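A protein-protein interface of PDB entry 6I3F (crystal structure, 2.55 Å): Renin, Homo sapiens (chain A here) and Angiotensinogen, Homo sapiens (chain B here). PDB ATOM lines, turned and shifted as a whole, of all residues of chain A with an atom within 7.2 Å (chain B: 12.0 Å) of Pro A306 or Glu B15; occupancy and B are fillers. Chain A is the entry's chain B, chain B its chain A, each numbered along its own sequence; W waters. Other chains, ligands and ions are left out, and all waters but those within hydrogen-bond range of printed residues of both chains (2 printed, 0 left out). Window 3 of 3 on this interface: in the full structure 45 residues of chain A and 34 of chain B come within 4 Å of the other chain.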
ATOM      1  N   ARG A  82      20.189 -18.050  24.721  1.00  0.00           N
ATOM      2  CA  ARG A  82      20.486 -18.143  23.265  1.00  0.00           C
ATOM      3  C   ARG A  82      21.789 -17.390  22.969  1.00  0.00           C
ATOM      4  O   ARG A  82      21.858 -16.184  23.280  1.00  0.00           O
ATOM      5  CB  ARG A  82      19.314 -17.586  22.449  1.00  0.00           C
ATOM      6  CG  ARG A  82      17.974 -18.243  22.756  1.00  0.00           C
ATOM      7  CD  ARG A  82      16.790 -17.510  22.150  1.00  0.00           C
ATOM      8  NE  ARG A  82      15.616 -17.561  23.016  1.00  0.00           N
ATOM      9  CZ  ARG A  82      14.694 -18.526  23.020  1.00  0.00           C
ATOM     10  NH1 ARG A  82      13.678 -18.456  23.867  1.00  0.00           N
ATOM     11  NH2 ARG A  82      14.782 -19.555  22.192  1.00  0.00           N
ATOM     12  N   TYR A  83      22.786 -18.091  22.420  1.00  0.00           N
ATOM     13  CA  TYR A  83      24.082 -17.530  21.951  1.00  0.00           C
ATOM     14  C   TYR A  83      24.082 -17.550  20.416  1.00  0.00           C
ATOM     15  O   TYR A  83      23.062 -17.967  19.835  1.00  0.00           O
ATOM     16  CB  TYR A  83      25.248 -18.298  22.579  1.00  0.00           C
ATOM     17  CG  TYR A  83      25.278 -18.247  24.087  1.00  0.00           C
ATOM     18  CD1 TYR A  83      25.665 -17.096  24.753  1.00  0.00           C
ATOM     19  CD2 TYR A  83      24.907 -19.342  24.852  1.00  0.00           C
ATOM     20  CE1 TYR A  83      25.687 -17.033  26.138  1.00  0.00           C
ATOM     21  CE2 TYR A  83      24.925 -19.297  26.237  1.00  0.00           C
ATOM     22  CZ  TYR A  83      25.317 -18.138  26.885  1.00  0.00           C
ATOM     23  OH  TYR A  83      25.336 -18.082  28.249  1.00  0.00           O
ATOM     24  N   THR A  87      22.511 -22.920  21.826  1.00  0.00           N
ATOM     25  CA  THR A  87      21.597 -22.520  22.930  1.00  0.00           C
ATOM     26  C   THR A  87      21.725 -23.531  24.074  1.00  0.00           C
ATOM     27  O   THR A  87      21.698 -24.740  23.782  1.00  0.00           O
ATOM     28  CB  THR A  87      20.152 -22.441  22.417  1.00  0.00           C
ATOM     29  OG1 THR A  87      20.086 -21.362  21.484  1.00  0.00           O
ATOM     30  CG2 THR A  87      19.128 -22.230  23.512  1.00  0.00           C
ATOM     31  N   MET A 303      31.266 -10.694  15.378  1.00  0.00           N
ATOM     32  CA  MET A 303      30.065 -11.096  16.156  1.00  0.00           C
ATOM     33  C   MET A 303      28.992 -10.011  16.000  1.00  0.00           C
ATOM     34  O   MET A 303      29.166  -8.915  16.566  1.00  0.00           O
ATOM     35  CB  MET A 303      30.408 -11.296  17.636  1.00  0.00           C
ATOM     36  CG  MET A 303      29.283 -11.920  18.445  1.00  0.00           C
ATOM     37  SD  MET A 303      28.643 -13.456  17.726  1.00  0.00           S
ATOM     38  CE  MET A 303      30.134 -14.446  17.652  1.00  0.00           C
ATOM     39  N   ASP A 304      27.943 -10.299  15.227  1.00  0.00           N
ATOM     40  CA  ASP A 304      26.792  -9.384  15.008  1.00  0.00           C
ATOM     41  C   ASP A 304      25.837  -9.525  16.198  1.00  0.00           C
ATOM     42  O   ASP A 304      24.956 -10.404  16.153  1.00  0.00           O
ATOM     43  CB  ASP A 304      26.108  -9.666  13.666  1.00  0.00           C
ATOM     44  CG  ASP A 304      26.948  -9.281  12.458  1.00  0.00           C
ATOM     45  OD1 ASP A 304      27.486  -8.155  12.453  1.00  0.00           O
ATOM     46  OD2 ASP A 304      27.061 -10.113  11.531  1.00  0.00           O
ATOM     47  N   ILE A 305      26.026  -8.702  17.233  1.00  0.00           N
ATOM     48  CA  ILE A 305      25.177  -8.692  18.460  1.00  0.00           C
ATOM     49  C   ILE A 305      23.866  -7.993  18.107  1.00  0.00           C
ATOM     50  O   ILE A 305      23.889  -6.874  17.598  1.00  0.00           O
ATOM     51  CB  ILE A 305      25.906  -8.019  19.640  1.00  0.00           C
ATOM     52  CG1 ILE A 305      27.216  -8.739  19.979  1.00  0.00           C
ATOM     53  CG2 ILE A 305      24.992  -7.919  20.853  1.00  0.00           C
ATOM     54  CD1 ILE A 305      28.183  -7.915  20.800  1.00  0.00           C
ATOM     55  N   PRO A 306      22.688  -8.618  18.346  1.00  0.00           N
ATOM     56  CA  PRO A 306      21.412  -8.036  17.935  1.00  0.00           C
ATOM     57  C   PRO A 306      20.994  -6.854  18.808  1.00  0.00           C
ATOM     58  O   PRO A 306      21.512  -6.679  19.910  1.00  0.00           O
ATOM     59  CB  PRO A 306      20.390  -9.176  18.087  1.00  0.00           C
ATOM     60  CG  PRO A 306      21.204 -10.411  18.432  1.00  0.00           C
ATOM     61  CD  PRO A 306      22.505  -9.908  19.022  1.00  0.00           C
ATOM     62  N   PRO A 307      20.053  -6.002  18.336  1.00  0.00           N
ATOM     63  CA  PRO A 307      19.448  -4.972  19.181  1.00  0.00           C
ATOM     64  C   PRO A 307      18.706  -5.588  20.365  1.00  0.00           C
ATOM     65  O   PRO A 307      18.274  -6.735  20.284  1.00  0.00           O
ATOM     66  CB  PRO A 307      18.463  -4.246  18.250  1.00  0.00           C
ATOM     67  CG  PRO A 307      18.935  -4.578  16.848  1.00  0.00           C
ATOM     68  CD  PRO A 307      19.551  -5.958  16.953  1.00  0.00           C
ATOM     69  N   PRO A 308      18.503  -4.856  21.485  1.00  0.00           N
ATOM     70  CA  PRO A 308      18.915  -3.456  21.611  1.00  0.00           C
ATOM     71  C   PRO A 308      20.391  -3.175  21.950  1.00  0.00           C
ATOM     72  O   PRO A 308      20.804  -2.046  21.765  1.00  0.00           O
ATOM     73  CB  PRO A 308      18.051  -2.965  22.783  1.00  0.00           C
ATOM     74  CG  PRO A 308      17.892  -4.190  23.658  1.00  0.00           C
ATOM     75  CD  PRO A 308      17.797  -5.344  22.682  1.00  0.00           C
ATOM     76  N   THR A 309      21.138  -4.171  22.443  1.00  0.00           N
ATOM     77  CA  THR A 309      22.551  -4.021  22.899  1.00  0.00           C
ATOM     78  C   THR A 309      23.451  -3.684  21.704  1.00  0.00           C
ATOM     79  O   THR A 309      24.323  -2.804  21.858  1.00  0.00           O
ATOM     80  CB  THR A 309      23.042  -5.276  23.632  1.00  0.00           C
ATOM     81  OG1 THR A 309      22.139  -5.527  24.710  1.00  0.00           O
ATOM     82  CG2 THR A 309      24.448  -5.137  24.175  1.00  0.00           C
ATOM     83  N   GLY A 310      23.250  -4.365  20.569  1.00  0.00           N
ATOM     84  CA  GLY A 310      24.011  -4.149  19.324  1.00  0.00           C
ATOM     85  C   GLY A 310      23.185  -3.417  18.267  1.00  0.00           C
ATOM     86  O   GLY A 310      22.031  -3.072  18.510  1.00  0.00           O
ATOM     87  N   PRO A 311      23.744  -3.146  17.062  1.00  0.00           N
ATOM     88  CA  PRO A 311      25.129  -3.492  16.735  1.00  0.00           C
ATOM     89  C   PRO A 311      26.137  -2.754  17.628  1.00  0.00           C
ATOM     90  O   PRO A 311      25.871  -1.627  18.001  1.00  0.00           O
ATOM     91  CB  PRO A 311      25.291  -3.056  15.269  1.00  0.00           C
ATOM     92  CG  PRO A 311      23.873  -2.962  14.746  1.00  0.00           C
ATOM     93  CD  PRO A 311      23.054  -2.504  15.934  1.00  0.00           C
ATOM     94  N   THR A 312      27.247  -3.413  17.960  1.00  0.00           N
ATOM     95  CA  THR A 312      28.279  -2.909  18.906  1.00  0.00           C
ATOM     96  C   THR A 312      29.572  -3.716  18.757  1.00  0.00           C
ATOM     97  O   THR A 312      29.498  -4.916  18.419  1.00  0.00           O
ATOM     98  CB  THR A 312      27.777  -2.968  20.356  1.00  0.00           C
ATOM     99  OG1 THR A 312      28.730  -2.312  21.194  1.00  0.00           O
ATOM    100  CG2 THR A 312      27.557  -4.381  20.855  1.00  0.00           C
ATOM    101  N   HIS B   9      32.229 -16.312  23.012  1.00  0.00           N
ATOM    102  CA  HIS B   9      31.415 -15.069  23.047  1.00  0.00           C
ATOM    103  C   HIS B   9      30.129 -15.376  23.816  1.00  0.00           C
ATOM    104  O   HIS B   9      29.254 -16.064  23.250  1.00  0.00           O
ATOM    105  CB  HIS B   9      31.162 -14.545  21.626  1.00  0.00           C
ATOM    106  CG  HIS B   9      31.091 -13.058  21.544  1.00  0.00           C
ATOM    107  ND1 HIS B   9      30.046 -12.336  22.088  1.00  0.00           N
ATOM    108  CD2 HIS B   9      31.928 -12.154  20.989  1.00  0.00           C
ATOM    109  CE1 HIS B   9      30.242 -11.052  21.871  1.00  0.00           C
ATOM    110  NE2 HIS B   9      31.389 -10.913  21.195  1.00  0.00           N
ATOM    111  N   LEU B  10      30.046 -14.916  25.067  1.00  0.00           N
ATOM    112  CA  LEU B  10      28.992 -15.300  26.043  1.00  0.00           C
ATOM    113  C   LEU B  10      28.008 -14.141  26.238  1.00  0.00           C
ATOM    114  O   LEU B  10      27.231 -14.189  27.209  1.00  0.00           O
ATOM    115  CB  LEU B  10      29.666 -15.703  27.358  1.00  0.00           C
ATOM    116  CG  LEU B  10      30.610 -16.902  27.266  1.00  0.00           C
ATOM    117  CD1 LEU B  10      31.361 -17.102  28.573  1.00  0.00           C
ATOM    118  CD2 LEU B  10      29.855 -18.168  26.887  1.00  0.00           C
ATOM    119  N   VAL B  11      28.028 -13.150  25.342  1.00  0.00           N
ATOM    120  CA  VAL B  11      26.952 -12.122  25.233  1.00  0.00           C
ATOM    121  C   VAL B  11      25.716 -12.840  24.689  1.00  0.00           C
ATOM    122  O   VAL B  11      25.846 -13.526  23.655  1.00  0.00           O
ATOM    123  CB  VAL B  11      27.364 -10.938  24.338  1.00  0.00           C
ATOM    124  CG1 VAL B  11      26.247  -9.909  24.224  1.00  0.00           C
ATOM    125  CG2 VAL B  11      28.647 -10.279  24.819  1.00  0.00           C
ATOM    126  N   ILE B  12      24.576 -12.716  25.375  1.00  0.00           N
ATOM    127  CA  ILE B  12      23.312 -13.439  25.040  1.00  0.00           C
ATOM    128  C   ILE B  12      22.574 -12.647  23.956  1.00  0.00           C
ATOM    129  O   ILE B  12      22.197 -11.488  24.216  1.00  0.00           O
ATOM    130  CB  ILE B  12      22.459 -13.679  26.303  1.00  0.00           C
ATOM    131  CG1 ILE B  12      23.129 -14.700  27.228  1.00  0.00           C
ATOM    132  CG2 ILE B  12      21.040 -14.098  25.941  1.00  0.00           C
ATOM    133  CD1 ILE B  12      22.517 -14.788  28.605  1.00  0.00           C
ATOM    134  N   HIS B  13      22.400 -13.263  22.784  1.00  0.00           N
ATOM    135  CA  HIS B  13      21.685 -12.706  21.604  1.00  0.00           C
ATOM    136  C   HIS B  13      20.188 -12.598  21.915  1.00  0.00           C
ATOM    137  O   HIS B  13      19.595 -11.544  21.612  1.00  0.00           O
ATOM    138  CB  HIS B  13      21.960 -13.568  20.363  1.00  0.00           C
ATOM    139  CG  HIS B  13      23.319 -13.358  19.785  1.00  0.00           C
ATOM    140  ND1 HIS B  13      23.538 -13.271  18.422  1.00  0.00           N
ATOM    141  CD2 HIS B  13      24.524 -13.191  20.373  1.00  0.00           C
ATOM    142  CE1 HIS B  13      24.821 -13.073  18.199  1.00  0.00           C
ATOM    143  NE2 HIS B  13      25.447 -13.018  19.380  1.00  0.00           N
ATOM    144  N   ASN B  14      19.617 -13.657  22.498  1.00  0.00           N
ATOM    145  CA  ASN B  14      18.178 -13.771  22.859  1.00  0.00           C
ATOM    146  C   ASN B  14      17.335 -13.776  21.572  1.00  0.00           C
ATOM    147  O   ASN B  14      16.268 -13.125  21.553  1.00  0.00           O
ATOM    148  CB  ASN B  14      17.762 -12.679  23.851  1.00  0.00           C
ATOM    149  CG  ASN B  14      16.419 -12.948  24.496  1.00  0.00           C
ATOM    150  OD1 ASN B  14      16.037 -14.102  24.681  1.00  0.00           O
ATOM    151  ND2 ASN B  14      15.698 -11.893  24.839  1.00  0.00           N
ATOM    152  N   GLU B  15      17.806 -14.494  20.543  1.00  0.00           N
ATOM    153  CA  GLU B  15      17.103 -14.712  19.247  1.00  0.00           C
ATOM    154  C   GLU B  15      17.460 -16.104  18.711  1.00  0.00           C
ATOM    155  O   GLU B  15      16.914 -16.465  17.648  1.00  0.00           O
ATOM    156  CB  GLU B  15      17.480 -13.629  18.234  1.00  0.00           C
ATOM    157  CG  GLU B  15      16.937 -12.252  18.579  1.00  0.00           C
ATOM    158  CD  GLU B  15      17.079 -11.219  17.474  1.00  0.00           C
ATOM    159  OE1 GLU B  15      17.889 -11.444  16.548  1.00  0.00           O
ATOM    160  OE2 GLU B  15      16.377 -10.192  17.540  1.00  0.00           O
HETATM  161  O   HOH W   1      26.479 -15.910  29.231  1.00  0.00           O
HETATM  162  O   HOH W   2      17.841 -16.073  25.526  1.00  0.00           O
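The backbone carbonyl oxygen of Arg A82 sits at hydrogen-bond distance from the backbone NH of His B13 (3.0 Å). N of Asn B14 is in hydrogen-bond range of O of Arg A82 (3.5 Å). The side-chain sulfur of Met A303 is in hydrogen-bond range of a ring nitrogen (NE2) of His B13 (3.6 Å).
Among the printed residues, merely in contact across the chains: Asp A304 with His B13 (3.4 Å), Tyr A83 with Leu B10 (3.4 Å), Arg A82 with Ile B12 (3.5 Å), Arg A82 with Glu B15 (3.6 Å), Pro A306 with His B13 (3.6 Å), Met A303 with His B9 (3.6 Å), Tyr A83 with Ile B12 (3.6 Å), Pro A306 with Glu B15 (3.7 Å), Tyr A83 with Val B11 (3.7 Å) and Ile A305 with His B9 (3.9 Å).
Of chain B, only Ile B12 (3.5 Å), His B13 (3.0 Å), Asn B14 (3.5 Å) and Glu B15 (3.6 Å) come within 4 Å of Arg A82. Of the printed residues of chain B, Tyr A83 touches Leu B10, Val B11 and Ile B12. Ile A305 touches just one residue of chain B: His B9 (3.9 Å). Of chain B, only His B13 and Glu B15 come within 4 Å of Pro A306. No residue of chain B comes within 4 Å of Pro A308. No residue of chain B comes within 4 Å of Gly A310. No residue of chain B comes within 4 Å of Pro A311. Of the printed residues of chain A, His B9 touches Met A303 (3.6 Å) and Ile A305 (3.9 Å). Of the printed residues of chain A, Leu B10 touches Tyr A83 (3.4 Å). Of chain A, only Arg A82 (3.6 Å) and Pro A306 (3.7 Å) come within 4 Å of Glu B15. The nearest printed residue of chain B that does not touch Pro A306 is Ile B12 (5.4 Å). The nearest residue of chain A that does not touch Glu B15 is Pro A307 (4.8 Å).
Printed residues of chain A that touch a printed residue of chain B: Arg A82, Tyr A83, Met A303, Asp A304, Ile A305 and Pro A306. Hydrophobic or aromatic side chains of chain A within 4 Å of the printed part of chain B: Tyr A83, Met A303, Ile A305 and Pro A306. Printed residues of chain B that touch a printed residue of chain A: His B9, Leu B10, Val B11, Ile B12, His B13, Asn B14 and Glu B15. Hydrophobic or aromatic side chains of chain B within 4 Å of the printed part of chain A: His B9, Ile B12 and His B13. Among the printed residues, 13 pairs touch across the chains.
Water W1 lies within hydrogen-bond range of the side-chain hydroxyl of Tyr A83 and the backbone carbonyl oxygen of Leu B10. Water W2 bridges the side-chain amide oxygen of Asn B14 and the backbone NH of Arg A82.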
